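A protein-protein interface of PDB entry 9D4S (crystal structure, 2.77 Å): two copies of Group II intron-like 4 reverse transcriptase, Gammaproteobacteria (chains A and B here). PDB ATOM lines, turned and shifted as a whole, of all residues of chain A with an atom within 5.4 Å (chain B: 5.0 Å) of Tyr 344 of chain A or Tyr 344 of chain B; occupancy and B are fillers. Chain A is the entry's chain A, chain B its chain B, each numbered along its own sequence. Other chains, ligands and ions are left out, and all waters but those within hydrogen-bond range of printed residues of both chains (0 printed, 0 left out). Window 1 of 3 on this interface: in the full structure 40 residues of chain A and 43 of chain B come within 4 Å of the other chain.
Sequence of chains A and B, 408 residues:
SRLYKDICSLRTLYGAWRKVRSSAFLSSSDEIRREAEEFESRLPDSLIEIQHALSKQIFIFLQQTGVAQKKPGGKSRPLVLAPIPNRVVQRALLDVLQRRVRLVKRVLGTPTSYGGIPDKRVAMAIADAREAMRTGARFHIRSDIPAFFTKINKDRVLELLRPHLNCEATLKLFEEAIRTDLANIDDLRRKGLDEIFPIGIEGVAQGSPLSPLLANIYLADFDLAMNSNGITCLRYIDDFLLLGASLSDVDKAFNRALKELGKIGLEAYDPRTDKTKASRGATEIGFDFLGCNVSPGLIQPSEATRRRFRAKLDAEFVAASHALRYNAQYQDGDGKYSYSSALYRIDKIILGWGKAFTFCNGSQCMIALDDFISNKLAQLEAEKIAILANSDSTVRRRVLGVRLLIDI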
ATOM      1  N   TYR A 339      22.924 -18.113  -9.633  1.00  0.00           N
ATOM      2  CA  TYR A 339      23.719 -18.934  -8.730  1.00  0.00           C
ATOM      3  C   TYR A 339      24.443 -18.100  -7.673  1.00  0.00           C
ATOM      4  O   TYR A 339      24.219 -18.267  -6.469  1.00  0.00           O
ATOM      5  CB  TYR A 339      24.695 -19.766  -9.555  1.00  0.00           C
ATOM      6  CG  TYR A 339      25.628 -20.621  -8.732  1.00  0.00           C
ATOM      7  CD1 TYR A 339      25.211 -21.844  -8.214  1.00  0.00           C
ATOM      8  CD2 TYR A 339      26.929 -20.211  -8.485  1.00  0.00           C
ATOM      9  CE1 TYR A 339      26.072 -22.637  -7.465  1.00  0.00           C
ATOM     10  CE2 TYR A 339      27.800 -20.995  -7.746  1.00  0.00           C
ATOM     11  CZ  TYR A 339      27.374 -22.206  -7.235  1.00  0.00           C
ATOM     12  OH  TYR A 339      28.258 -22.975  -6.496  1.00  0.00           O
ATOM     13  N   SER A 340      25.251 -17.141  -8.118  1.00  0.00           N
ATOM     14  CA  SER A 340      25.979 -16.299  -7.176  1.00  0.00           C
ATOM     15  C   SER A 340      25.026 -15.546  -6.245  1.00  0.00           C
ATOM     16  O   SER A 340      25.258 -15.487  -5.036  1.00  0.00           O
ATOM     17  CB  SER A 340      26.882 -15.320  -7.931  1.00  0.00           C
ATOM     18  OG  SER A 340      26.119 -14.471  -8.782  1.00  0.00           O
ATOM     19  N   SER A 341      23.968 -14.926  -6.789  1.00  0.00           N
ATOM     20  CA  SER A 341      23.050 -14.182  -5.928  1.00  0.00           C
ATOM     21  C   SER A 341      22.210 -15.107  -5.056  1.00  0.00           C
ATOM     22  O   SER A 341      21.907 -14.765  -3.906  1.00  0.00           O
ATOM     23  CB  SER A 341      22.115 -13.273  -6.734  1.00  0.00           C
ATOM     24  OG  SER A 341      22.727 -12.036  -7.054  1.00  0.00           O
ATOM     25  N   ALA A 342      21.847 -16.284  -5.574  1.00  0.00           N
ATOM     26  CA  ALA A 342      21.069 -17.240  -4.791  1.00  0.00           C
ATOM     27  C   ALA A 342      21.877 -17.761  -3.609  1.00  0.00           C
ATOM     28  O   ALA A 342      21.428 -17.695  -2.460  1.00  0.00           O
ATOM     29  CB  ALA A 342      20.599 -18.394  -5.681  1.00  0.00           C
ATOM     30  N   LEU A 343      23.071 -18.296  -3.875  1.00  0.00           N
ATOM     31  CA  LEU A 343      23.900 -18.771  -2.775  1.00  0.00           C
ATOM     32  C   LEU A 343      24.192 -17.661  -1.774  1.00  0.00           C
ATOM     33  O   LEU A 343      24.198 -17.901  -0.556  1.00  0.00           O
ATOM     34  CB  LEU A 343      25.193 -19.368  -3.323  1.00  0.00           C
ATOM     35  CG  LEU A 343      25.131 -20.898  -3.369  1.00  0.00           C
ATOM     36  CD1 LEU A 343      24.002 -21.375  -4.242  1.00  0.00           C
ATOM     37  CD2 LEU A 343      26.445 -21.510  -3.822  1.00  0.00           C
ATOM     38  N   TYR A 344      24.396 -16.438  -2.242  1.00  0.00           N
ATOM     39  CA  TYR A 344      24.739 -15.327  -1.317  1.00  0.00           C
ATOM     40  C   TYR A 344      23.572 -15.079  -0.355  1.00  0.00           C
ATOM     41  O   TYR A 344      23.811 -14.886   0.840  1.00  0.00           O
ATOM     42  CB  TYR A 344      25.107 -14.072  -2.110  1.00  0.00           C
ATOM     43  CG  TYR A 344      25.386 -12.843  -1.289  1.00  0.00           C
ATOM     44  CD1 TYR A 344      24.367 -11.993  -0.894  1.00  0.00           C
ATOM     45  CD2 TYR A 344      26.679 -12.504  -0.933  1.00  0.00           C
ATOM     46  CE1 TYR A 344      24.622 -10.855  -0.148  1.00  0.00           C
ATOM     47  CE2 TYR A 344      26.951 -11.371  -0.186  1.00  0.00           C
ATOM     48  CZ  TYR A 344      25.918 -10.543   0.208  1.00  0.00           C
ATOM     49  OH  TYR A 344      26.178  -9.417   0.944  1.00  0.00           O
ATOM     50  N   ARG A 345      22.347 -15.086  -0.869  1.00  0.00           N
ATOM     51  CA  ARG A 345      21.158 -14.792  -0.034  1.00  0.00           C
ATOM     52  C   ARG A 345      20.917 -15.950   0.941  1.00  0.00           C
ATOM     53  O   ARG A 345      20.672 -15.684   2.121  1.00  0.00           O
ATOM     54  CB  ARG A 345      19.962 -14.542  -0.953  1.00  0.00           C
ATOM     55  CG  ARG A 345      18.601 -14.744  -0.304  1.00  0.00           C
ATOM     56  CD  ARG A 345      17.469 -14.235  -1.177  1.00  0.00           C
ATOM     57  NE  ARG A 345      17.085 -15.174  -2.220  1.00  0.00           N
ATOM     58  CZ  ARG A 345      17.512 -15.114  -3.473  1.00  0.00           C
ATOM     59  NH1 ARG A 345      17.930 -13.967  -3.976  1.00  0.00           N
ATOM     60  NH2 ARG A 345      17.520 -16.204  -4.220  1.00  0.00           N
ATOM     61  N   ILE A 346      20.989 -17.182   0.446  1.00  0.00           N
ATOM     62  CA  ILE A 346      20.817 -18.361   1.333  1.00  0.00           C
ATOM     63  C   ILE A 346      21.810 -18.209   2.486  1.00  0.00           C
ATOM     64  O   ILE A 346      21.418 -18.460   3.627  1.00  0.00           O
ATOM     65  CB  ILE A 346      21.009 -19.666   0.543  1.00  0.00           C
ATOM     66  CG1 ILE A 346      19.844 -19.910  -0.418  1.00  0.00           C
ATOM     67  CG2 ILE A 346      21.217 -20.846   1.477  1.00  0.00           C
ATOM     68  CD1 ILE A 346      20.058 -21.060  -1.369  1.00  0.00           C
ATOM     69  N   ASP A 347      23.038 -17.781   2.195  1.00  0.00           N
ATOM     70  CA  ASP A 347      23.988 -17.660   3.296  1.00  0.00           C
ATOM     71  C   ASP A 347      23.471 -16.707   4.362  1.00  0.00           C
ATOM     72  O   ASP A 347      23.539 -17.016   5.556  1.00  0.00           O
ATOM     73  CB  ASP A 347      25.350 -17.186   2.773  1.00  0.00           C
ATOM     74  CG  ASP A 347      26.349 -16.922   3.896  1.00  0.00           C
ATOM     75  OD1 ASP A 347      26.977 -17.883   4.389  1.00  0.00           O
ATOM     76  OD2 ASP A 347      26.508 -15.750   4.294  1.00  0.00           O
ATOM     77  N   LYS A 348      22.917 -15.567   3.949  1.00  0.00           N
ATOM     78  CA  LYS A 348      22.437 -14.576   4.902  1.00  0.00           C
ATOM     79  C   LYS A 348      21.144 -15.018   5.587  1.00  0.00           C
ATOM     80  O   LYS A 348      20.859 -14.574   6.701  1.00  0.00           O
ATOM     81  CB  LYS A 348      22.240 -13.232   4.198  1.00  0.00           C
ATOM     82  CG  LYS A 348      23.438 -12.779   3.388  1.00  0.00           C
ATOM     83  CD  LYS A 348      24.664 -12.630   4.278  1.00  0.00           C
ATOM     84  CE  LYS A 348      25.860 -12.184   3.490  1.00  0.00           C
ATOM     85  NZ  LYS A 348      26.377 -13.287   2.629  1.00  0.00           N
ATOM     86  N   TYR B 339      33.338 -17.945  -2.919  1.00  0.00           N
ATOM     87  CA  TYR B 339      32.929 -17.969  -4.341  1.00  0.00           C
ATOM     88  C   TYR B 339      31.642 -17.166  -4.505  1.00  0.00           C
ATOM     89  O   TYR B 339      31.587 -16.295  -5.376  1.00  0.00           O
ATOM     90  CB  TYR B 339      32.732 -19.413  -4.800  1.00  0.00           C
ATOM     91  CG  TYR B 339      32.629 -19.596  -6.293  1.00  0.00           C
ATOM     92  CD1 TYR B 339      33.707 -19.332  -7.119  1.00  0.00           C
ATOM     93  CD2 TYR B 339      31.450 -20.012  -6.884  1.00  0.00           C
ATOM     94  CE1 TYR B 339      33.623 -19.493  -8.489  1.00  0.00           C
ATOM     95  CE2 TYR B 339      31.345 -20.176  -8.253  1.00  0.00           C
ATOM     96  CZ  TYR B 339      32.437 -19.915  -9.060  1.00  0.00           C
ATOM     97  OH  TYR B 339      32.352 -20.069 -10.418  1.00  0.00           O
ATOM     98  N   SER B 340      30.648 -17.435  -3.668  1.00  0.00           N
ATOM     99  CA  SER B 340      29.335 -16.759  -3.804  1.00  0.00           C
ATOM    100  C   SER B 340      29.503 -15.256  -3.598  1.00  0.00           C
ATOM    101  O   SER B 340      28.963 -14.487  -4.394  1.00  0.00           O
ATOM    102  CB  SER B 340      28.362 -17.328  -2.816  1.00  0.00           C
ATOM    103  OG  SER B 340      28.846 -17.168  -1.493  1.00  0.00           O
ATOM    104  N   SER B 341      30.222 -14.876  -2.549  1.00  0.00           N
ATOM    105  CA  SER B 341      30.391 -13.446  -2.210  1.00  0.00           C
ATOM    106  C   SER B 341      31.236 -12.733  -3.258  1.00  0.00           C
ATOM    107  O   SER B 341      30.912 -11.589  -3.593  1.00  0.00           O
ATOM    108  CB  SER B 341      30.988 -13.301  -0.854  1.00  0.00           C
ATOM    109  OG  SER B 341      30.295 -14.098   0.093  1.00  0.00           O
ATOM    110  N   ALA B 342      32.310 -13.375  -3.702  1.00  0.00           N
ATOM    111  CA  ALA B 342      33.208 -12.710  -4.662  1.00  0.00           C
ATOM    112  C   ALA B 342      32.488 -12.445  -5.978  1.00  0.00           C
ATOM    113  O   ALA B 342      32.541 -11.315  -6.461  1.00  0.00           O
ATOM    114  CB  ALA B 342      34.392 -13.599  -4.899  1.00  0.00           C
ATOM    115  N   LEU B 343      31.757 -13.442  -6.460  1.00  0.00           N
ATOM    116  CA  LEU B 343      31.006 -13.287  -7.722  1.00  0.00           C
ATOM    117  C   LEU B 343      29.947 -12.209  -7.506  1.00  0.00           C
ATOM    118  O   LEU B 343      29.738 -11.410  -8.421  1.00  0.00           O
ATOM    119  CB  LEU B 343      30.410 -14.640  -8.118  1.00  0.00           C
ATOM    120  CG  LEU B 343      31.411 -15.675  -8.620  1.00  0.00           C
ATOM    121  CD1 LEU B 343      30.728 -16.696  -9.515  1.00  0.00           C
ATOM    122  CD2 LEU B 343      32.561 -15.006  -9.356  1.00  0.00           C
ATOM    123  N   TYR B 344      29.313 -12.210  -6.338  1.00  0.00           N
ATOM    124  CA  TYR B 344      28.281 -11.195  -6.016  1.00  0.00           C
ATOM    125  C   TYR B 344      28.944  -9.820  -6.010  1.00  0.00           C
ATOM    126  O   TYR B 344      28.391  -8.906  -6.627  1.00  0.00           O
ATOM    127  CB  TYR B 344      27.594 -11.532  -4.689  1.00  0.00           C
ATOM    128  CG  TYR B 344      26.408 -10.680  -4.326  1.00  0.00           C
ATOM    129  CD1 TYR B 344      26.568  -9.428  -3.763  1.00  0.00           C
ATOM    130  CD2 TYR B 344      25.120 -11.132  -4.545  1.00  0.00           C
ATOM    131  CE1 TYR B 344      25.480  -8.642  -3.426  1.00  0.00           C
ATOM    132  CE2 TYR B 344      24.019 -10.362  -4.215  1.00  0.00           C
ATOM    133  CZ  TYR B 344      24.202  -9.112  -3.654  1.00  0.00           C
ATOM    134  OH  TYR B 344      23.115  -8.344  -3.330  1.00  0.00           O
ATOM    135  N   ARG B 345      30.098  -9.687  -5.356  1.00  0.00           N
ATOM    136  CA  ARG B 345      30.755  -8.384  -5.445  1.00  0.00           C
ATOM    137  C   ARG B 345      31.168  -8.059  -6.875  1.00  0.00           C
ATOM    138  O   ARG B 345      30.984  -6.927  -7.348  1.00  0.00           O
ATOM    139  CB  ARG B 345      31.994  -8.355  -4.564  1.00  0.00           C
ATOM    140  CG  ARG B 345      31.861  -7.705  -3.210  1.00  0.00           C
ATOM    141  CD  ARG B 345      33.213  -7.113  -2.794  1.00  0.00           C
ATOM    142  NE  ARG B 345      34.329  -7.998  -3.124  1.00  0.00           N
ATOM    143  CZ  ARG B 345      34.433  -9.275  -2.771  1.00  0.00           C
ATOM    144  NH1 ARG B 345      33.632  -9.811  -1.860  1.00  0.00           N
ATOM    145  NH2 ARG B 345      35.388 -10.023  -3.324  1.00  0.00           N
ATOM    146  N   ILE B 346      31.708  -9.045  -7.589  1.00  0.00           N
ATOM    147  CA  ILE B 346      32.225  -8.752  -8.912  1.00  0.00           C
ATOM    148  C   ILE B 346      31.068  -8.343  -9.811  1.00  0.00           C
ATOM    149  O   ILE B 346      31.168  -7.364 -10.565  1.00  0.00           O
ATOM    150  CB  ILE B 346      33.017  -9.964  -9.445  1.00  0.00           C
ATOM    151  CG1 ILE B 346      34.427  -9.974  -8.817  1.00  0.00           C
ATOM    152  CG2 ILE B 346      33.071  -9.972 -10.971  1.00  0.00           C
ATOM    153  CD1 ILE B 346      35.109 -11.346  -8.684  1.00  0.00           C
ATOM    154  N   ASP B 347      29.917  -9.002  -9.647  1.00  0.00           N
ATOM    155  CA  ASP B 347      28.737  -8.654 -10.428  1.00  0.00           C
ATOM    156  C   ASP B 347      28.293  -7.215 -10.176  1.00  0.00           C
ATOM    157  O   ASP B 347      27.935  -6.492 -11.119  1.00  0.00           O
ATOM    158  CB  ASP B 347      27.600  -9.618 -10.117  1.00  0.00           C
ATOM    159  CG  ASP B 347      26.344  -9.270 -10.863  1.00  0.00           C
ATOM    160  OD1 ASP B 347      26.200  -9.764 -11.993  1.00  0.00           O
ATOM    161  OD2 ASP B 347      25.516  -8.493 -10.333  1.00  0.00           O
ATOM    162  N   LYS B 348      28.281  -6.792  -8.910  1.00  0.00           N
ATOM    163  CA  LYS B 348      27.874  -5.425  -8.593  1.00  0.00           C
ATOM    164  C   LYS B 348      28.946  -4.398  -8.968  1.00  0.00           C
ATOM    165  O   LYS B 348      28.622  -3.229  -9.193  1.00  0.00           O
ATOM    166  CB  LYS B 348      27.531  -5.315  -7.108  1.00  0.00           C
ATOM    167  CG  LYS B 348      26.551  -6.373  -6.625  1.00  0.00           C
ATOM    168  CD  LYS B 348      25.256  -6.378  -7.429  1.00  0.00           C
ATOM    169  CE  LYS B 348      24.339  -7.495  -6.949  1.00  0.00           C
ATOM    170  NZ  LYS B 348      24.923  -8.851  -7.168  1.00  0.00           N
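The side-chain carboxylate (OD2) of Asp 347 of chain B lies within salt-bridge range of the side-chain amino group (NZ) of Lys 348 of chain B, 3.2 Å away.
Among the printed residues, pairs that only touch across the chains: Tyr 339 of chain A with Tyr 339 of chain B (3.7 Å), Ser 340 of chain A with Ser 340 of chain B (3.9 Å), Ser 340 of chain A with Leu 343 of chain B (3.6 Å), Ser 341 of chain A with Tyr 344 of chain B (3.5 Å), Ser 341 of chain A with Lys 348 of chain B (3.9 Å), Leu 343 of chain A with Ser 340 of chain B (3.8 Å) and Tyr 344 of chain A with Tyr 344 of chain B (3.7 Å).
Tyr 344 of chain A touches just one residue of chain B: Tyr 344. Tyr 344 of chain B touches two residues of chain A. Of the printed residues of chain A, Ser 340 of chain B touches Ser 340 (3.9 Å) and Leu 343 (3.8 Å). Of the printed residues of chain B, Ser 340 of chain A touches Ser 340 and Leu 343. Printed residues of chain A within 4 Å of Tyr 339 of chain B: Tyr 339 (3.7 Å). Of the printed residues of chain B, Ser 341 of chain A touches Tyr 344 and Lys 348.
Printed residues of chain A that touch a printed residue of chain B: Tyr 339, Ser 340, Ser 341, Leu 343 and Tyr 344. Hydrophobic or aromatic side chains of chain A within 4 Å of the printed part of chain B: Tyr 339, Leu 343 and Tyr 344. Of the 10 printed residues of chain B, 5 touch a printed residue of chain A. Among the printed residues, 7 pairs touch across the chains.
Tyr 339 of chain A touches its own counterpart, Tyr 339 of chain B. Ser 340 of chain A touches its own counterpart, Ser 340 of chain B. Ser 340 of chain A touches Leu 343 of chain B, and with the chains exchanged Leu 343 of chain A touches Ser 340 of chain B. Tyr 344 of chain A touches its own counterpart, Tyr 344 of chain B. 10 positions are printed for both chains.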
